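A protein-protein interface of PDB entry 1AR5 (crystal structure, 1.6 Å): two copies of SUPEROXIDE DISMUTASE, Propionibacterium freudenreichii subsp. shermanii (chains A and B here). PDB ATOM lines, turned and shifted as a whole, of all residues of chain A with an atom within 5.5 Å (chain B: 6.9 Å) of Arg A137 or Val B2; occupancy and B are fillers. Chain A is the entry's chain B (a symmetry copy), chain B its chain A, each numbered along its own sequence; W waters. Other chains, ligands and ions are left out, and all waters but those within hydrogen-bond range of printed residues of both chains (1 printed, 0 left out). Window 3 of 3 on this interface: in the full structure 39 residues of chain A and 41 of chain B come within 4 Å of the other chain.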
ATOM      1  N   PHE A 103       8.258 -16.126  17.482  1.00  0.00           N
ATOM      2  CA  PHE A 103       9.544 -15.439  17.405  1.00  0.00           C
ATOM      3  C   PHE A 103      10.633 -15.875  18.389  1.00  0.00           C
ATOM      4  O   PHE A 103      11.798 -15.525  18.206  1.00  0.00           O
ATOM      5  CB  PHE A 103       9.325 -13.926  17.481  1.00  0.00           C
ATOM      6  CG  PHE A 103       8.427 -13.397  16.399  1.00  0.00           C
ATOM      7  CD1 PHE A 103       8.731 -13.617  15.059  1.00  0.00           C
ATOM      8  CD2 PHE A 103       7.263 -12.706  16.718  1.00  0.00           C
ATOM      9  CE1 PHE A 103       7.885 -13.161  14.051  1.00  0.00           C
ATOM     10  CE2 PHE A 103       6.409 -12.244  15.716  1.00  0.00           C
ATOM     11  CZ  PHE A 103       6.721 -12.474  14.382  1.00  0.00           C
ATOM     12  N   VAL A 130      10.597  -5.319  21.749  1.00  0.00           N
ATOM     13  CA  VAL A 130      10.029  -4.363  20.803  1.00  0.00           C
ATOM     14  C   VAL A 130       9.412  -5.001  19.568  1.00  0.00           C
ATOM     15  O   VAL A 130       9.681  -6.157  19.240  1.00  0.00           O
ATOM     16  CB  VAL A 130      11.109  -3.368  20.284  1.00  0.00           C
ATOM     17  CG1 VAL A 130      11.715  -2.575  21.426  1.00  0.00           C
ATOM     18  CG2 VAL A 130      12.194  -4.119  19.520  1.00  0.00           C
ATOM     19  N   TRP A 131       8.567  -4.227  18.898  1.00  0.00           N
ATOM     20  CA  TRP A 131       7.950  -4.660  17.660  1.00  0.00           C
ATOM     21  C   TRP A 131       8.771  -3.983  16.569  1.00  0.00           C
ATOM     22  O   TRP A 131       8.954  -2.766  16.577  1.00  0.00           O
ATOM     23  CB  TRP A 131       6.488  -4.210  17.563  1.00  0.00           C
ATOM     24  CG  TRP A 131       5.886  -4.447  16.193  1.00  0.00           C
ATOM     25  CD1 TRP A 131       5.591  -3.501  15.252  1.00  0.00           C
ATOM     26  CD2 TRP A 131       5.531  -5.711  15.612  1.00  0.00           C
ATOM     27  NE1 TRP A 131       5.082  -4.095  14.125  1.00  0.00           N
ATOM     28  CE2 TRP A 131       5.032  -5.450  14.316  1.00  0.00           C
ATOM     29  CE3 TRP A 131       5.585  -7.037  16.059  1.00  0.00           C
ATOM     30  CZ2 TRP A 131       4.587  -6.467  13.464  1.00  0.00           C
ATOM     31  CZ3 TRP A 131       5.144  -8.049  15.211  1.00  0.00           C
ATOM     32  CH2 TRP A 131       4.652  -7.755  13.928  1.00  0.00           C
ATOM     33  N   ASP A 132       9.307  -4.803  15.674  1.00  0.00           N
ATOM     34  CA  ASP A 132      10.109  -4.358  14.545  1.00  0.00           C
ATOM     35  C   ASP A 132       9.162  -4.277  13.346  1.00  0.00           C
ATOM     36  O   ASP A 132       8.739  -5.299  12.821  1.00  0.00           O
ATOM     37  CB  ASP A 132      11.228  -5.384  14.314  1.00  0.00           C
ATOM     38  CG  ASP A 132      11.938  -5.220  12.978  1.00  0.00           C
ATOM     39  OD1 ASP A 132      11.878  -4.138  12.357  1.00  0.00           O
ATOM     40  OD2 ASP A 132      12.574  -6.203  12.553  1.00  0.00           O
ATOM     41  N   PRO A 133       8.821  -3.051  12.904  1.00  0.00           N
ATOM     42  CA  PRO A 133       7.924  -2.772  11.774  1.00  0.00           C
ATOM     43  C   PRO A 133       8.460  -3.220  10.415  1.00  0.00           C
ATOM     44  O   PRO A 133       7.688  -3.529   9.508  1.00  0.00           O
ATOM     45  CB  PRO A 133       7.790  -1.247  11.808  1.00  0.00           C
ATOM     46  CG  PRO A 133       8.154  -0.876  13.220  1.00  0.00           C
ATOM     47  CD  PRO A 133       9.296  -1.794  13.503  1.00  0.00           C
ATOM     48  N   GLY A 135      10.842  -5.842   9.860  1.00  0.00           N
ATOM     49  CA  GLY A 135      10.844  -7.292   9.790  1.00  0.00           C
ATOM     50  C   GLY A 135       9.538  -7.917  10.256  1.00  0.00           C
ATOM     51  O   GLY A 135       9.363  -9.132  10.143  1.00  0.00           O
ATOM     52  N   LYS A 136       8.627  -7.087  10.768  1.00  0.00           N
ATOM     53  CA  LYS A 136       7.325  -7.535  11.273  1.00  0.00           C
ATOM     54  C   LYS A 136       7.492  -8.682  12.265  1.00  0.00           C
ATOM     55  O   LYS A 136       6.891  -9.747  12.123  1.00  0.00           O
ATOM     56  CB  LYS A 136       6.411  -7.947  10.118  1.00  0.00           C
ATOM     57  CG  LYS A 136       5.897  -6.781   9.299  1.00  0.00           C
ATOM     58  CD  LYS A 136       5.130  -7.272   8.090  1.00  0.00           C
ATOM     59  CE  LYS A 136       4.262  -6.174   7.503  1.00  0.00           C
ATOM     60  NZ  LYS A 136       3.550  -6.631   6.274  1.00  0.00           N
ATOM     61  N   ARG A 137       8.295  -8.434  13.294  1.00  0.00           N
ATOM     62  CA  ARG A 137       8.582  -9.441  14.303  1.00  0.00           C
ATOM     63  C   ARG A 137       8.861  -8.794  15.651  1.00  0.00           C
ATOM     64  O   ARG A 137       8.987  -7.575  15.750  1.00  0.00           O
ATOM     65  CB  ARG A 137       9.810 -10.255  13.876  1.00  0.00           C
ATOM     66  CG  ARG A 137      11.075  -9.413  13.682  1.00  0.00           C
ATOM     67  CD  ARG A 137      12.266 -10.247  13.227  1.00  0.00           C
ATOM     68  NE  ARG A 137      12.636 -11.266  14.204  1.00  0.00           N
ATOM     69  CZ  ARG A 137      12.576 -12.574  13.986  1.00  0.00           C
ATOM     70  NH1 ARG A 137      12.160 -13.041  12.819  1.00  0.00           N
ATOM     71  NH2 ARG A 137      12.930 -13.420  14.941  1.00  0.00           N
ATOM     72  N   ILE A 138       8.925  -9.619  16.689  1.00  0.00           N
ATOM     73  CA  ILE A 138       9.220  -9.141  18.032  1.00  0.00           C
ATOM     74  C   ILE A 138      10.676  -9.489  18.322  1.00  0.00           C
ATOM     75  O   ILE A 138      11.079 -10.646  18.201  1.00  0.00           O
ATOM     76  CB  ILE A 138       8.315  -9.811  19.095  1.00  0.00           C
ATOM     77  CG1 ILE A 138       6.843  -9.489  18.818  1.00  0.00           C
ATOM     78  CG2 ILE A 138       8.706  -9.339  20.492  1.00  0.00           C
ATOM     79  CD1 ILE A 138       5.880 -10.102  19.816  1.00  0.00           C
ATOM     80  N   ASN A 139      11.463  -8.475  18.671  1.00  0.00           N
ATOM     81  CA  ASN A 139      12.881  -8.656  18.981  1.00  0.00           C
ATOM     82  C   ASN A 139      13.180  -8.164  20.392  1.00  0.00           C
ATOM     83  O   ASN A 139      12.370  -7.463  20.993  1.00  0.00           O
ATOM     84  CB  ASN A 139      13.755  -7.819  18.032  1.00  0.00           C
ATOM     85  CG  ASN A 139      13.733  -8.310  16.593  1.00  0.00           C
ATOM     86  OD1 ASN A 139      13.859  -7.516  15.663  1.00  0.00           O
ATOM     87  ND2 ASN A 139      13.616  -9.616  16.406  1.00  0.00           N
ATOM     88  N   ALA B   1      15.201 -15.014   3.715  1.00  0.00           N
ATOM     89  CA  ALA B   1      15.763 -14.326   4.910  1.00  0.00           C
ATOM     90  C   ALA B   1      14.731 -13.372   5.496  1.00  0.00           C
ATOM     91  O   ALA B   1      13.720 -13.073   4.859  1.00  0.00           O
ATOM     92  CB  ALA B   1      17.026 -13.565   4.527  1.00  0.00           C
ATOM     93  N   VAL B   2      14.988 -12.896   6.711  1.00  0.00           N
ATOM     94  CA  VAL B   2      14.081 -11.964   7.370  1.00  0.00           C
ATOM     95  C   VAL B   2      14.171 -10.588   6.711  1.00  0.00           C
ATOM     96  O   VAL B   2      13.156  -9.994   6.351  1.00  0.00           O
ATOM     97  CB  VAL B   2      14.405 -11.837   8.877  1.00  0.00           C
ATOM     98  CG1 VAL B   2      13.493 -10.813   9.539  1.00  0.00           C
ATOM     99  CG2 VAL B   2      14.258 -13.187   9.555  1.00  0.00           C
ATOM    100  N   TYR B   3      15.397 -10.106   6.526  1.00  0.00           N
ATOM    101  CA  TYR B   3      15.632  -8.803   5.919  1.00  0.00           C
ATOM    102  C   TYR B   3      16.168  -8.951   4.505  1.00  0.00           C
ATOM    103  O   TYR B   3      16.925  -9.876   4.209  1.00  0.00           O
ATOM    104  CB  TYR B   3      16.608  -7.986   6.771  1.00  0.00           C
ATOM    105  CG  TYR B   3      16.141  -7.804   8.199  1.00  0.00           C
ATOM    106  CD1 TYR B   3      15.003  -7.051   8.491  1.00  0.00           C
ATOM    107  CD2 TYR B   3      16.818  -8.410   9.257  1.00  0.00           C
ATOM    108  CE1 TYR B   3      14.546  -6.910   9.800  1.00  0.00           C
ATOM    109  CE2 TYR B   3      16.371  -8.275  10.572  1.00  0.00           C
ATOM    110  CZ  TYR B   3      15.234  -7.526  10.835  1.00  0.00           C
ATOM    111  OH  TYR B   3      14.779  -7.403  12.130  1.00  0.00           O
ATOM    112  N   THR B   4      15.740  -8.047   3.630  1.00  0.00           N
ATOM    113  CA  THR B   4      16.170  -8.056   2.239  1.00  0.00           C
ATOM    114  C   THR B   4      16.585  -6.659   1.810  1.00  0.00           C
ATOM    115  O   THR B   4      16.078  -5.661   2.328  1.00  0.00           O
ATOM    116  CB  THR B   4      15.051  -8.556   1.290  1.00  0.00           C
ATOM    117  OG1 THR B   4      13.883  -7.743   1.449  1.00  0.00           O
ATOM    118  CG2 THR B   4      14.699 -10.004   1.587  1.00  0.00           C
ATOM    119  N   VAL B  36      22.189  -5.533   5.819  1.00  0.00           N
ATOM    120  CA  VAL B  36      21.122  -6.520   5.687  1.00  0.00           C
ATOM    121  C   VAL B  36      21.649  -7.898   6.087  1.00  0.00           C
ATOM    122  O   VAL B  36      21.005  -8.613   6.856  1.00  0.00           O
ATOM    123  CB  VAL B  36      20.574  -6.568   4.242  1.00  0.00           C
ATOM    124  CG1 VAL B  36      19.566  -7.699   4.091  1.00  0.00           C
ATOM    125  CG2 VAL B  36      19.933  -5.238   3.885  1.00  0.00           C
ATOM    126  N   ALA B  39      22.261  -7.954   9.909  1.00  0.00           N
ATOM    127  CA  ALA B  39      21.038  -8.049  10.703  1.00  0.00           C
ATOM    128  C   ALA B  39      20.495  -9.480  10.678  1.00  0.00           C
ATOM    129  O   ALA B  39      20.042  -9.998  11.697  1.00  0.00           O
ATOM    130  CB  ALA B  39      19.993  -7.071  10.182  1.00  0.00           C
ATOM    131  N   ASN B  40      20.566 -10.121   9.512  1.00  0.00           N
ATOM    132  CA  ASN B  40      20.094 -11.491   9.365  1.00  0.00           C
ATOM    133  C   ASN B  40      20.956 -12.445  10.173  1.00  0.00           C
ATOM    134  O   ASN B  40      20.443 -13.362  10.814  1.00  0.00           O
ATOM    135  CB  ASN B  40      20.106 -11.911   7.894  1.00  0.00           C
ATOM    136  CG  ASN B  40      18.921 -11.372   7.127  1.00  0.00           C
ATOM    137  OD1 ASN B  40      17.814 -11.278   7.657  1.00  0.00           O
ATOM    138  ND2 ASN B  40      19.141 -11.023   5.865  1.00  0.00           N
ATOM    139  N   LEU B  43      20.182 -12.290  13.942  1.00  0.00           N
ATOM    140  CA  LEU B  43      18.979 -13.039  14.296  1.00  0.00           C
ATOM    141  C   LEU B  43      19.241 -14.544  14.326  1.00  0.00           C
ATOM    142  O   LEU B  43      18.740 -15.242  15.208  1.00  0.00           O
ATOM    143  CB  LEU B  43      17.829 -12.725  13.336  1.00  0.00           C
ATOM    144  CG  LEU B  43      17.172 -11.344  13.429  1.00  0.00           C
ATOM    145  CD1 LEU B  43      16.035 -11.266  12.424  1.00  0.00           C
ATOM    146  CD2 LEU B  43      16.653 -11.093  14.836  1.00  0.00           C
ATOM    147  N   ASP B  44      20.031 -15.038  13.373  1.00  0.00           N
ATOM    148  CA  ASP B  44      20.362 -16.462  13.321  1.00  0.00           C
ATOM    149  C   ASP B  44      21.160 -16.874  14.554  1.00  0.00           C
ATOM    150  O   ASP B  44      20.965 -17.959  15.103  1.00  0.00           O
ATOM    151  CB  ASP B  44      21.176 -16.788  12.062  1.00  0.00           C
ATOM    152  CG  ASP B  44      20.331 -16.808  10.800  1.00  0.00           C
ATOM    153  OD1 ASP B  44      19.099 -17.004  10.896  1.00  0.00           O
ATOM    154  OD2 ASP B  44      20.907 -16.643   9.703  1.00  0.00           O
ATOM    155  N   ARG B  50      19.254 -19.374  21.846  1.00  0.00           N
ATOM    156  CA  ARG B  50      18.063 -19.860  22.537  1.00  0.00           C
ATOM    157  C   ARG B  50      17.992 -21.381  22.543  1.00  0.00           C
ATOM    158  O   ARG B  50      17.663 -21.983  23.562  1.00  0.00           O
ATOM    159  CB  ARG B  50      16.787 -19.300  21.900  1.00  0.00           C
ATOM    160  CG  ARG B  50      16.536 -17.828  22.165  1.00  0.00           C
ATOM    161  CD  ARG B  50      15.136 -17.413  21.712  1.00  0.00           C
ATOM    162  NE  ARG B  50      14.912 -17.620  20.281  1.00  0.00           N
ATOM    163  CZ  ARG B  50      15.203 -16.729  19.336  1.00  0.00           C
ATOM    164  NH1 ARG B  50      15.737 -15.557  19.657  1.00  0.00           N
ATOM    165  NH2 ARG B  50      14.956 -17.010  18.064  1.00  0.00           N
ATOM    166  N   HIS B  72      20.124  -0.684   8.240  1.00  0.00           N
ATOM    167  CA  HIS B  72      19.187  -1.113   7.206  1.00  0.00           C
ATOM    168  C   HIS B  72      17.987  -0.164   7.161  1.00  0.00           C
ATOM    169  O   HIS B  72      17.607   0.308   6.094  1.00  0.00           O
ATOM    170  CB  HIS B  72      18.739  -2.552   7.490  1.00  0.00           C
ATOM    171  CG  HIS B  72      17.755  -3.095   6.498  1.00  0.00           C
ATOM    172  ND1 HIS B  72      16.842  -4.076   6.824  1.00  0.00           N
ATOM    173  CD2 HIS B  72      17.544  -2.803   5.196  1.00  0.00           C
ATOM    174  CE1 HIS B  72      16.111  -4.363   5.764  1.00  0.00           C
ATOM    175  NE2 HIS B  72      16.515  -3.605   4.762  1.00  0.00           N
HETATM  176  O   HOH W   1      12.778 -16.155  15.529  1.00  0.00           O
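No position is printed for both chains.
OH of Tyr B3 lies within hydrogen-bond range of OD2 of Asp A132, at 2.5 Å. NH2 of Arg B50 sits at hydrogen-bond distance from O of Phe A103, 3.5 Å away.
The side-chain amide oxygen of Asn B40 sits at hydrogen-bond distance from the backbone NH of Val B2 (3.4 Å). OD1 of Asn B40 sits at hydrogen-bond distance from N of Tyr B3, 2.9 Å away. The backbone carbonyl oxygen of Asn A139 sits at hydrogen-bond distance from the backbone NH of Val A130, 2.9 Å away. OD1 of Asp A132 is in hydrogen-bond range of N of Gly A135 (3.2 Å). The backbone NH (N) of Asp A132 lies within hydrogen-bond range of the backbone carbonyl oxygen (O) of Arg A137 (2.8 Å). The guanidinium group of Arg A137 sits close to the side-chain amide nitrogen of Asn A139 (2.9 Å).
Water W1 lies within hydrogen-bond range of NH2 of Arg A137 (2.8 Å), O of Phe A103 (2.9 Å) and NH2 of Arg B50 (3.4 Å).
Gly A135 touches Tyr B3 (CA to CE1, 3.7 Å). Arg A137 touches Val B2 (NH1 to CG2, 3.9 Å). CD of Arg A137 touches OH of Tyr B3, at 3.95 Å. NE of Arg A137 touches CD1 of Leu B43 (3.8 Å). OD1 of Asn A139 touches OH of Tyr B3 (3.7 Å). ND2 of Asn A139 touches CD2 of Leu B43 (3.7 Å).
Of the printed residues of chain B, Arg A137 touches Val B2, Tyr B3 and Leu B43. Of chain A, only Arg A137 (3.9 Å) comes within 4 Å of Val B2. Of the printed residues of chain A, Leu B43 touches Arg A137 and Asn A139. Printed residues of chain A within 4 Å of Arg B50: Phe A103. Printed residues of chain A within 4 Å of Tyr B3: Asp A132, Gly A135, Arg A137 and Asn A139. Of the printed residues of chain B, Phe A103 touches Arg B50. Of the printed residues of chain B, Asp A132 touches Tyr B3 (2.5 Å). The nearest residue of chain B that does not touch Arg A137 is Arg B50 (5.2 Å). The nearest residue of chain A that does not touch Val B2 is Gly A135 (4.4 Å). The nearest printed residue of chain B that does not touch Phe A103 is Leu B43 (7.4 Å).
Of the 10 printed residues of chain A, 5 touch a printed residue of chain B.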
